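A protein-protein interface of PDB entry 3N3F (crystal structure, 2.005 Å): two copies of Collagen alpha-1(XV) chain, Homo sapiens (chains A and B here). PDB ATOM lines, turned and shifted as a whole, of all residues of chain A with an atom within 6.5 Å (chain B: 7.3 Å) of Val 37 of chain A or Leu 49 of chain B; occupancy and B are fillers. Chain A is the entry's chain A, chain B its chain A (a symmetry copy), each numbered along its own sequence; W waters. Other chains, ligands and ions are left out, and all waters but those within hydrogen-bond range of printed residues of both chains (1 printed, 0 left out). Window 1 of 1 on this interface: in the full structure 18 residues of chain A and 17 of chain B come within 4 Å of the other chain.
Hydrophobic or aromatic side chains of chain B within 4 Å of the printed part of chain A: Tyr 26, Phe 33, Leu 46, Leu 49, Ile 50 and Ile 52.
Along chain B the printed residues that touch a printed residue of chain A span positions 26 to 52.
Hydrophobic or aromatic side chains of chain A that line the printed part of chain B: Ile 35, Val 37 and Trp 41.
Along chain A the printed residues that touch a printed residue of chain B span positions 21 to 42.
Among the printed residues, no Asp or Glu carboxylate lies within 4 Å of a Lys or Arg side-chain nitrogen of the other chain.
No position is printed for both chains.
Water W1 bridges O of Asp 39 of chain A (2.6 Å) and N of Ile 52 of chain B (3.1 Å).
N of Arg 38 of chain A sits at hydrogen-bond distance from OH of Tyr 26 of chain B (3.4 Å).
The backbone NH (N) of Ile 52 of chain B lies close to the backbone carbonyl oxygen (O) of Asp 39 of chain A.
O of Trp 41 of chain A is in hydrogen-bond range of N of Ile 50 of chain B (2.8 Å).
NZ of Lys 42 of chain A lies within hydrogen-bond range of O of Ser 30 of chain B (3.5 Å).
NZ of Lys 42 of chain A lies within hydrogen-bond range of OG1 of Thr 31 of chain B (2.8 Å).
The side-chain carboxylate of Glu 21 of chain A sits close to the side-chain hydroxyl of Tyr 26 of chain B (2.4 Å).
Phe 33 of chain B touches Ile 35 of chain A.
NH2 of Arg 36 of chain A touches CD1 of Ile 52 of chain B (3.5 Å).
Val 37 of chain A touches Tyr 26 of chain B (CB to OH, 3.6 Å).
Leu 49 of chain B touches Val 37 of chain A.
Pro 51 of chain B touches Asp 39 of chain A (CA to O, 3.8 Å).
O of Ile 50 of chain B touches CA of Gly 40 of chain A (3.2 Å).
Gly 40 of chain A touches Ile 52 of chain B.
Pro 51 of chain B touches Trp 41 of chain A (O to CZ3, 3.8 Å).
Trp 41 of chain A touches Ile 52 of chain B (CZ3 to CA, 3.6 Å).
Lys 42 of chain A touches Gly 47 of chain B (CG to O, 3.6 Å).
The backbone NH of Arg 38 of chain A sits close to the side-chain carboxylate of Glu 21 of chain A.
N of Gly 22 of chain A sits at hydrogen-bond distance from O of Arg 36 of chain A.
The backbone carbonyl oxygen (O) of Thr 23 of chain A sits at hydrogen-bond distance from the backbone NH (N) of Arg 36 of chain A, 2.8 Å away.
N of Ile 35 of chain A is in hydrogen-bond range of O of Lys 42 of chain A (2.9 Å).
O of Gly 40 of chain A sits close to NH1 of Arg 36 of chain A, at 3.4 Å.
OG of Ser 30 of chain B sits at hydrogen-bond distance from OE1 of Glu 32 of chain B (3.1 Å).
Of the printed residues of chain B, Val 37 of chain A touches Tyr 26 and Leu 49.
Leu 49 of chain B touches two residues of chain A.
Of the printed residues of chain B, Ile 35 of chain A touches Phe 33 and Leu 46.
Of the printed residues of chain B, Asp 39 of chain A touches Pro 51 and Ile 52.
Printed residues of chain B within 4 Å of Glu 21 of chain A: Tyr 26 (2.4 Å).
Of the printed residues of chain A, Ile 50 of chain B touches Gly 40 (3.2 Å) and Trp 41 (2.8 Å).
Printed residues of chain B within 4 Å of Arg 38 of chain A: Tyr 26 (3.4 Å) and Thr 31 (3.8 Å).
Ile 20 of chain A touches none of the printed residues of chain B.
The nearest printed residue of chain B that does not touch Val 37 of chain A is Thr 31 of chain B (4.01 Å).
The nearest printed residue of chain A that does not touch Leu 49 of chain B is Lys 42 of chain A (4.03 Å).
The nearest printed residue of chain A that does not touch Thr 31 of chain B is Val 37 of chain A (4.01 Å).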
ATOM      1  N   ILE A  20     -11.645  16.137  21.306  1.00  0.00           N
ATOM      2  CA  ILE A  20     -12.912  15.635  21.825  1.00  0.00           C
ATOM      3  C   ILE A  20     -13.461  16.567  22.896  1.00  0.00           C
ATOM      4  O   ILE A  20     -12.711  17.130  23.692  1.00  0.00           O
ATOM      5  CB  ILE A  20     -12.757  14.224  22.449  1.00  0.00           C
ATOM      6  CG1 ILE A  20     -12.236  13.235  21.402  1.00  0.00           C
ATOM      7  CG2 ILE A  20     -14.103  13.743  22.990  1.00  0.00           C
ATOM      8  CD1 ILE A  20     -13.198  12.982  20.264  1.00  0.00           C
ATOM      9  N   GLU A  21     -14.776  16.732  22.899  1.00  0.00           N
ATOM     10  CA  GLU A  21     -15.444  17.570  23.881  1.00  0.00           C
ATOM     11  C   GLU A  21     -14.975  17.168  25.281  1.00  0.00           C
ATOM     12  O   GLU A  21     -14.754  15.989  25.551  1.00  0.00           O
ATOM     13  CB  GLU A  21     -16.959  17.387  23.736  1.00  0.00           C
ATOM     14  CG  GLU A  21     -17.796  17.742  24.950  1.00  0.00           C
ATOM     15  CD  GLU A  21     -19.288  17.636  24.664  1.00  0.00           C
ATOM     16  OE1 GLU A  21     -19.699  16.677  23.978  1.00  0.00           O
ATOM     17  OE2 GLU A  21     -20.049  18.506  25.128  1.00  0.00           O
ATOM     18  N   GLY A  22     -14.802  18.150  26.159  1.00  0.00           N
ATOM     19  CA  GLY A  22     -14.359  17.860  27.513  1.00  0.00           C
ATOM     20  C   GLY A  22     -12.854  17.733  27.674  1.00  0.00           C
ATOM     21  O   GLY A  22     -12.382  17.242  28.699  1.00  0.00           O
ATOM     22  N   THR A  23     -12.100  18.172  26.667  1.00  0.00           N
ATOM     23  CA  THR A  23     -10.639  18.112  26.701  1.00  0.00           C
ATOM     24  C   THR A  23     -10.072  19.503  26.961  1.00  0.00           C
ATOM     25  O   THR A  23     -10.656  20.502  26.548  1.00  0.00           O
ATOM     26  CB  THR A  23     -10.060  17.601  25.354  1.00  0.00           C
ATOM     27  OG1 THR A  23     -10.498  16.261  25.116  1.00  0.00           O
ATOM     28  CG2 THR A  23      -8.539  17.631  25.374  1.00  0.00           C
ATOM     29  N   ILE A  35     -11.080  25.013  26.850  1.00  0.00           N
ATOM     30  CA  ILE A  35     -11.679  23.706  27.040  1.00  0.00           C
ATOM     31  C   ILE A  35     -12.575  23.468  25.840  1.00  0.00           C
ATOM     32  O   ILE A  35     -13.338  24.344  25.445  1.00  0.00           O
ATOM     33  CB  ILE A  35     -12.537  23.642  28.315  1.00  0.00           C
ATOM     34  CG1 ILE A  35     -13.569  24.768  28.299  1.00  0.00           C
ATOM     35  CG2 ILE A  35     -11.654  23.742  29.540  1.00  0.00           C
ATOM     36  CD1 ILE A  35     -14.703  24.559  29.257  1.00  0.00           C
ATOM     37  N   ARG A  36     -12.458  22.287  25.252  1.00  0.00           N
ATOM     38  CA  ARG A  36     -13.263  21.916  24.103  1.00  0.00           C
ATOM     39  C   ARG A  36     -14.627  21.483  24.649  1.00  0.00           C
ATOM     40  O   ARG A  36     -14.708  20.563  25.461  1.00  0.00           O
ATOM     41  CB  ARG A  36     -12.599  20.746  23.373  1.00  0.00           C
ATOM     42  CG  ARG A  36     -12.553  20.866  21.865  1.00  0.00           C
ATOM     43  CD  ARG A  36     -13.915  21.122  21.303  1.00  0.00           C
ATOM     44  NE  ARG A  36     -14.050  20.671  19.925  1.00  0.00           N
ATOM     45  CZ  ARG A  36     -15.201  20.702  19.265  1.00  0.00           C
ATOM     46  NH1 ARG A  36     -16.283  21.167  19.871  1.00  0.00           N
ATOM     47  NH2 ARG A  36     -15.278  20.256  18.020  1.00  0.00           N
ATOM     48  N   VAL A  37     -15.690  22.156  24.230  1.00  0.00           N
ATOM     49  CA  VAL A  37     -17.025  21.794  24.696  1.00  0.00           C
ATOM     50  C   VAL A  37     -17.961  21.571  23.520  1.00  0.00           C
ATOM     51  O   VAL A  37     -17.544  21.584  22.366  1.00  0.00           O
ATOM     52  CB  VAL A  37     -17.635  22.882  25.607  1.00  0.00           C
ATOM     53  CG1 VAL A  37     -16.734  23.116  26.806  1.00  0.00           C
ATOM     54  CG2 VAL A  37     -17.841  24.165  24.829  1.00  0.00           C
ATOM     55  N   ARG A  38     -19.233  21.361  23.821  1.00  0.00           N
ATOM     56  CA  ARG A  38     -20.219  21.140  22.778  1.00  0.00           C
ATOM     57  C   ARG A  38     -20.372  22.390  21.911  1.00  0.00           C
ATOM     58  O   ARG A  38     -20.708  23.467  22.407  1.00  0.00           O
ATOM     59  CB  ARG A  38     -21.563  20.774  23.409  1.00  0.00           C
ATOM     60  CG  ARG A  38     -22.687  20.516  22.423  1.00  0.00           C
ATOM     61  CD  ARG A  38     -23.967  20.208  23.181  1.00  0.00           C
ATOM     62  NE  ARG A  38     -24.302  21.281  24.115  1.00  0.00           N
ATOM     63  CZ  ARG A  38     -25.196  21.174  25.093  1.00  0.00           C
ATOM     64  NH1 ARG A  38     -25.855  20.038  25.275  1.00  0.00           N
ATOM     65  NH2 ARG A  38     -25.432  22.208  25.891  1.00  0.00           N
ATOM     66  N   ASP A  39     -20.109  22.225  20.617  1.00  0.00           N
ATOM     67  CA  ASP A  39     -20.219  23.294  19.628  1.00  0.00           C
ATOM     68  C   ASP A  39     -19.176  24.400  19.713  1.00  0.00           C
ATOM     69  O   ASP A  39     -19.391  25.500  19.205  1.00  0.00           O
ATOM     70  CB  ASP A  39     -21.620  23.908  19.672  1.00  0.00           C
ATOM     71  CG  ASP A  39     -22.713  22.870  19.500  1.00  0.00           C
ATOM     72  OD1 ASP A  39     -22.616  22.053  18.560  1.00  0.00           O
ATOM     73  OD2 ASP A  39     -23.670  22.876  20.300  1.00  0.00           O
ATOM     74  N   GLY A  40     -18.042  24.119  20.345  1.00  0.00           N
ATOM     75  CA  GLY A  40     -17.012  25.137  20.423  1.00  0.00           C
ATOM     76  C   GLY A  40     -16.003  24.954  21.534  1.00  0.00           C
ATOM     77  O   GLY A  40     -15.633  23.837  21.883  1.00  0.00           O
ATOM     78  N   TRP A  41     -15.557  26.080  22.077  1.00  0.00           N
ATOM     79  CA  TRP A  41     -14.586  26.099  23.156  1.00  0.00           C
ATOM     80  C   TRP A  41     -14.993  27.184  24.140  1.00  0.00           C
ATOM     81  O   TRP A  41     -15.839  28.030  23.845  1.00  0.00           O
ATOM     82  CB  TRP A  41     -13.189  26.458  22.636  1.00  0.00           C
ATOM     83  CG  TRP A  41     -12.695  25.676  21.456  1.00  0.00           C
ATOM     84  CD1 TRP A  41     -11.807  24.639  21.473  1.00  0.00           C
ATOM     85  CD2 TRP A  41     -13.006  25.916  20.081  1.00  0.00           C
ATOM     86  NE1 TRP A  41     -11.538  24.224  20.191  1.00  0.00           N
ATOM     87  CE2 TRP A  41     -12.262  24.992  19.316  1.00  0.00           C
ATOM     88  CE3 TRP A  41     -13.841  26.829  19.417  1.00  0.00           C
ATOM     89  CZ2 TRP A  41     -12.326  24.950  17.917  1.00  0.00           C
ATOM     90  CZ3 TRP A  41     -13.904  26.786  18.024  1.00  0.00           C
ATOM     91  CH2 TRP A  41     -13.150  25.854  17.292  1.00  0.00           C
ATOM     92  N   LYS A  42     -14.372  27.151  25.311  1.00  0.00           N
ATOM     93  CA  LYS A  42     -14.589  28.150  26.348  1.00  0.00           C
ATOM     94  C   LYS A  42     -13.221  28.410  26.955  1.00  0.00           C
ATOM     95  O   LYS A  42     -12.474  27.474  27.235  1.00  0.00           O
ATOM     96  CB  LYS A  42     -15.555  27.640  27.418  1.00  0.00           C
ATOM     97  CG  LYS A  42     -17.021  27.687  27.011  1.00  0.00           C
ATOM     98  CD  LYS A  42     -17.921  27.276  28.170  1.00  0.00           C
ATOM     99  CE  LYS A  42     -19.382  27.493  27.842  1.00  0.00           C
ATOM    100  NZ  LYS A  42     -20.268  27.113  28.979  1.00  0.00           N
ATOM    101  N   TYR B  26     -17.059  17.689  34.229  1.00  0.00           N
ATOM    102  CA  TYR B  26     -17.725  18.366  33.125  1.00  0.00           C
ATOM    103  C   TYR B  26     -19.228  18.145  33.209  1.00  0.00           C
ATOM    104  O   TYR B  26     -19.685  17.025  33.426  1.00  0.00           O
ATOM    105  CB  TYR B  26     -17.190  17.817  31.798  1.00  0.00           C
ATOM    106  CG  TYR B  26     -17.823  18.377  30.536  1.00  0.00           C
ATOM    107  CD1 TYR B  26     -17.842  19.749  30.287  1.00  0.00           C
ATOM    108  CD2 TYR B  26     -18.299  17.523  29.541  1.00  0.00           C
ATOM    109  CE1 TYR B  26     -18.307  20.255  29.073  1.00  0.00           C
ATOM    110  CE2 TYR B  26     -18.766  18.018  28.324  1.00  0.00           C
ATOM    111  CZ  TYR B  26     -18.761  19.385  28.096  1.00  0.00           C
ATOM    112  OH  TYR B  26     -19.172  19.876  26.881  1.00  0.00           O
ATOM    113  N   LEU B  27     -19.998  19.217  33.063  1.00  0.00           N
ATOM    114  CA  LEU B  27     -21.451  19.099  33.085  1.00  0.00           C
ATOM    115  C   LEU B  27     -21.904  19.218  31.637  1.00  0.00           C
ATOM    116  O   LEU B  27     -21.860  20.298  31.048  1.00  0.00           O
ATOM    117  CB  LEU B  27     -22.075  20.202  33.944  1.00  0.00           C
ATOM    118  CG  LEU B  27     -21.619  20.227  35.409  1.00  0.00           C
ATOM    119  CD1 LEU B  27     -22.504  21.183  36.190  1.00  0.00           C
ATOM    120  CD2 LEU B  27     -21.707  18.826  36.016  1.00  0.00           C
ATOM    121  N   SER B  30     -24.846  21.978  30.656  1.00  0.00           N
ATOM    122  CA  SER B  30     -24.479  23.388  30.680  1.00  0.00           C
ATOM    123  C   SER B  30     -23.061  23.666  30.168  1.00  0.00           C
ATOM    124  O   SER B  30     -22.629  24.818  30.121  1.00  0.00           O
ATOM    125  CB  SER B  30     -24.623  23.927  32.104  1.00  0.00           C
ATOM    126  OG  SER B  30     -23.821  23.191  33.011  1.00  0.00           O
ATOM    127  N   THR B  31     -22.354  22.612  29.774  1.00  0.00           N
ATOM    128  CA  THR B  31     -20.983  22.724  29.285  1.00  0.00           C
ATOM    129  C   THR B  31     -20.146  23.547  30.261  1.00  0.00           C
ATOM    130  O   THR B  31     -19.418  24.459  29.868  1.00  0.00           O
ATOM    131  CB  THR B  31     -20.911  23.357  27.865  1.00  0.00           C
ATOM    132  OG1 THR B  31     -21.277  24.740  27.918  1.00  0.00           O
ATOM    133  CG2 THR B  31     -21.845  22.625  26.913  1.00  0.00           C
ATOM    134  N   GLU B  32     -20.276  23.222  31.544  1.00  0.00           N
ATOM    135  CA  GLU B  32     -19.529  23.903  32.590  1.00  0.00           C
ATOM    136  C   GLU B  32     -18.569  22.917  33.230  1.00  0.00           C
ATOM    137  O   GLU B  32     -18.678  21.706  33.031  1.00  0.00           O
ATOM    138  CB  GLU B  32     -20.474  24.466  33.654  1.00  0.00           C
ATOM    139  CG  GLU B  32     -21.389  25.558  33.141  1.00  0.00           C
ATOM    140  CD  GLU B  32     -22.221  26.191  34.239  1.00  0.00           C
ATOM    141  OE1 GLU B  32     -22.954  25.456  34.935  1.00  0.00           O
ATOM    142  OE2 GLU B  32     -22.143  27.426  34.400  1.00  0.00           O
ATOM    143  N   PHE B  33     -17.624  23.440  34.001  1.00  0.00           N
ATOM    144  CA  PHE B  33     -16.645  22.594  34.656  1.00  0.00           C
ATOM    145  C   PHE B  33     -16.535  22.892  36.137  1.00  0.00           C
ATOM    146  O   PHE B  33     -16.597  24.045  36.562  1.00  0.00           O
ATOM    147  CB  PHE B  33     -15.277  22.772  33.995  1.00  0.00           C
ATOM    148  CG  PHE B  33     -14.838  21.591  33.174  1.00  0.00           C
ATOM    149  CD1 PHE B  33     -14.222  20.499  33.778  1.00  0.00           C
ATOM    150  CD2 PHE B  33     -15.031  21.574  31.797  1.00  0.00           C
ATOM    151  CE1 PHE B  33     -13.800  19.403  33.019  1.00  0.00           C
ATOM    152  CE2 PHE B  33     -14.615  20.485  31.028  1.00  0.00           C
ATOM    153  CZ  PHE B  33     -13.998  19.399  31.641  1.00  0.00           C
ATOM    154  N   LEU B  46     -15.189  29.880  33.560  1.00  0.00           N
ATOM    155  CA  LEU B  46     -15.050  29.737  32.114  1.00  0.00           C
ATOM    156  C   LEU B  46     -15.645  30.930  31.382  1.00  0.00           C
ATOM    157  O   LEU B  46     -16.565  31.580  31.875  1.00  0.00           O
ATOM    158  CB  LEU B  46     -15.743  28.462  31.641  1.00  0.00           C
ATOM    159  CG  LEU B  46     -15.207  27.142  32.189  1.00  0.00           C
ATOM    160  CD1 LEU B  46     -16.062  25.992  31.684  1.00  0.00           C
ATOM    161  CD2 LEU B  46     -13.771  26.970  31.763  1.00  0.00           C
ATOM    162  N   GLY B  47     -15.113  31.206  30.198  1.00  0.00           N
ATOM    163  CA  GLY B  47     -15.606  32.318  29.414  1.00  0.00           C
ATOM    164  C   GLY B  47     -16.828  31.959  28.591  1.00  0.00           C
ATOM    165  O   GLY B  47     -17.353  30.848  28.679  1.00  0.00           O
ATOM    166  N   GLU B  48     -17.280  32.918  27.791  1.00  0.00           N
ATOM    167  CA  GLU B  48     -18.439  32.745  26.922  1.00  0.00           C
ATOM    168  C   GLU B  48     -18.095  31.722  25.843  1.00  0.00           C
ATOM    169  O   GLU B  48     -16.932  31.580  25.460  1.00  0.00           O
ATOM    170  CB  GLU B  48     -18.786  34.085  26.269  1.00  0.00           C
ATOM    171  CG  GLU B  48     -20.266  34.338  26.061  1.00  0.00           C
ATOM    172  CD  GLU B  48     -21.005  34.597  27.362  1.00  0.00           C
ATOM    173  OE1 GLU B  48     -22.194  34.969  27.301  1.00  0.00           O
ATOM    174  OE2 GLU B  48     -20.401  34.429  28.443  1.00  0.00           O
ATOM    175  N   LEU B  49     -19.105  31.018  25.345  1.00  0.00           N
ATOM    176  CA  LEU B  49     -18.898  30.015  24.309  1.00  0.00           C
ATOM    177  C   LEU B  49     -18.325  30.608  23.025  1.00  0.00           C
ATOM    178  O   LEU B  49     -18.851  31.579  22.485  1.00  0.00           O
ATOM    179  CB  LEU B  49     -20.212  29.306  23.982  1.00  0.00           C
ATOM    180  CG  LEU B  49     -20.135  28.292  22.836  1.00  0.00           C
ATOM    181  CD1 LEU B  49     -19.238  27.128  23.236  1.00  0.00           C
ATOM    182  CD2 LEU B  49     -21.531  27.798  22.499  1.00  0.00           C
ATOM    183  N   ILE B  50     -17.237  30.017  22.546  1.00  0.00           N
ATOM    184  CA  ILE B  50     -16.607  30.462  21.312  1.00  0.00           C
ATOM    185  C   ILE B  50     -17.081  29.485  20.248  1.00  0.00           C
ATOM    186  O   ILE B  50     -16.635  28.335  20.203  1.00  0.00           O
ATOM    187  CB  ILE B  50     -15.074  30.410  21.414  1.00  0.00           C
ATOM    188  CG1 ILE B  50     -14.614  31.263  22.597  1.00  0.00           C
ATOM    189  CG2 ILE B  50     -14.449  30.900  20.117  1.00  0.00           C
ATOM    190  CD1 ILE B  50     -13.155  31.101  22.939  1.00  0.00           C
ATOM    191  N   PRO B  51     -18.020  29.924  19.393  1.00  0.00           N
ATOM    192  CA  PRO B  51     -18.585  29.107  18.318  1.00  0.00           C
ATOM    193  C   PRO B  51     -17.536  28.598  17.342  1.00  0.00           C
ATOM    194  O   PRO B  51     -16.553  29.283  17.060  1.00  0.00           O
ATOM    195  CB  PRO B  51     -19.580  30.057  17.649  1.00  0.00           C
ATOM    196  CG  PRO B  51     -19.985  30.970  18.767  1.00  0.00           C
ATOM    197  CD  PRO B  51     -18.660  31.250  19.427  1.00  0.00           C
ATOM    198  N   ILE B  52     -17.752  27.392  16.830  1.00  0.00           N
ATOM    199  CA  ILE B  52     -16.829  26.785  15.882  1.00  0.00           C
ATOM    200  C   ILE B  52     -16.944  27.472  14.520  1.00  0.00           C
ATOM    201  O   ILE B  52     -18.047  27.746  14.046  1.00  0.00           O
ATOM    202  CB  ILE B  52     -17.123  25.276  15.710  1.00  0.00           C
ATOM    203  CG1 ILE B  52     -16.928  24.550  17.041  1.00  0.00           C
ATOM    204  CG2 ILE B  52     -16.213  24.681  14.645  1.00  0.00           C
ATOM    205  CD1 ILE B  52     -17.187  23.059  16.980  1.00  0.00           C
HETATM  206  O   HOH W   1     -20.711  26.834  17.451  1.00  0.00           O
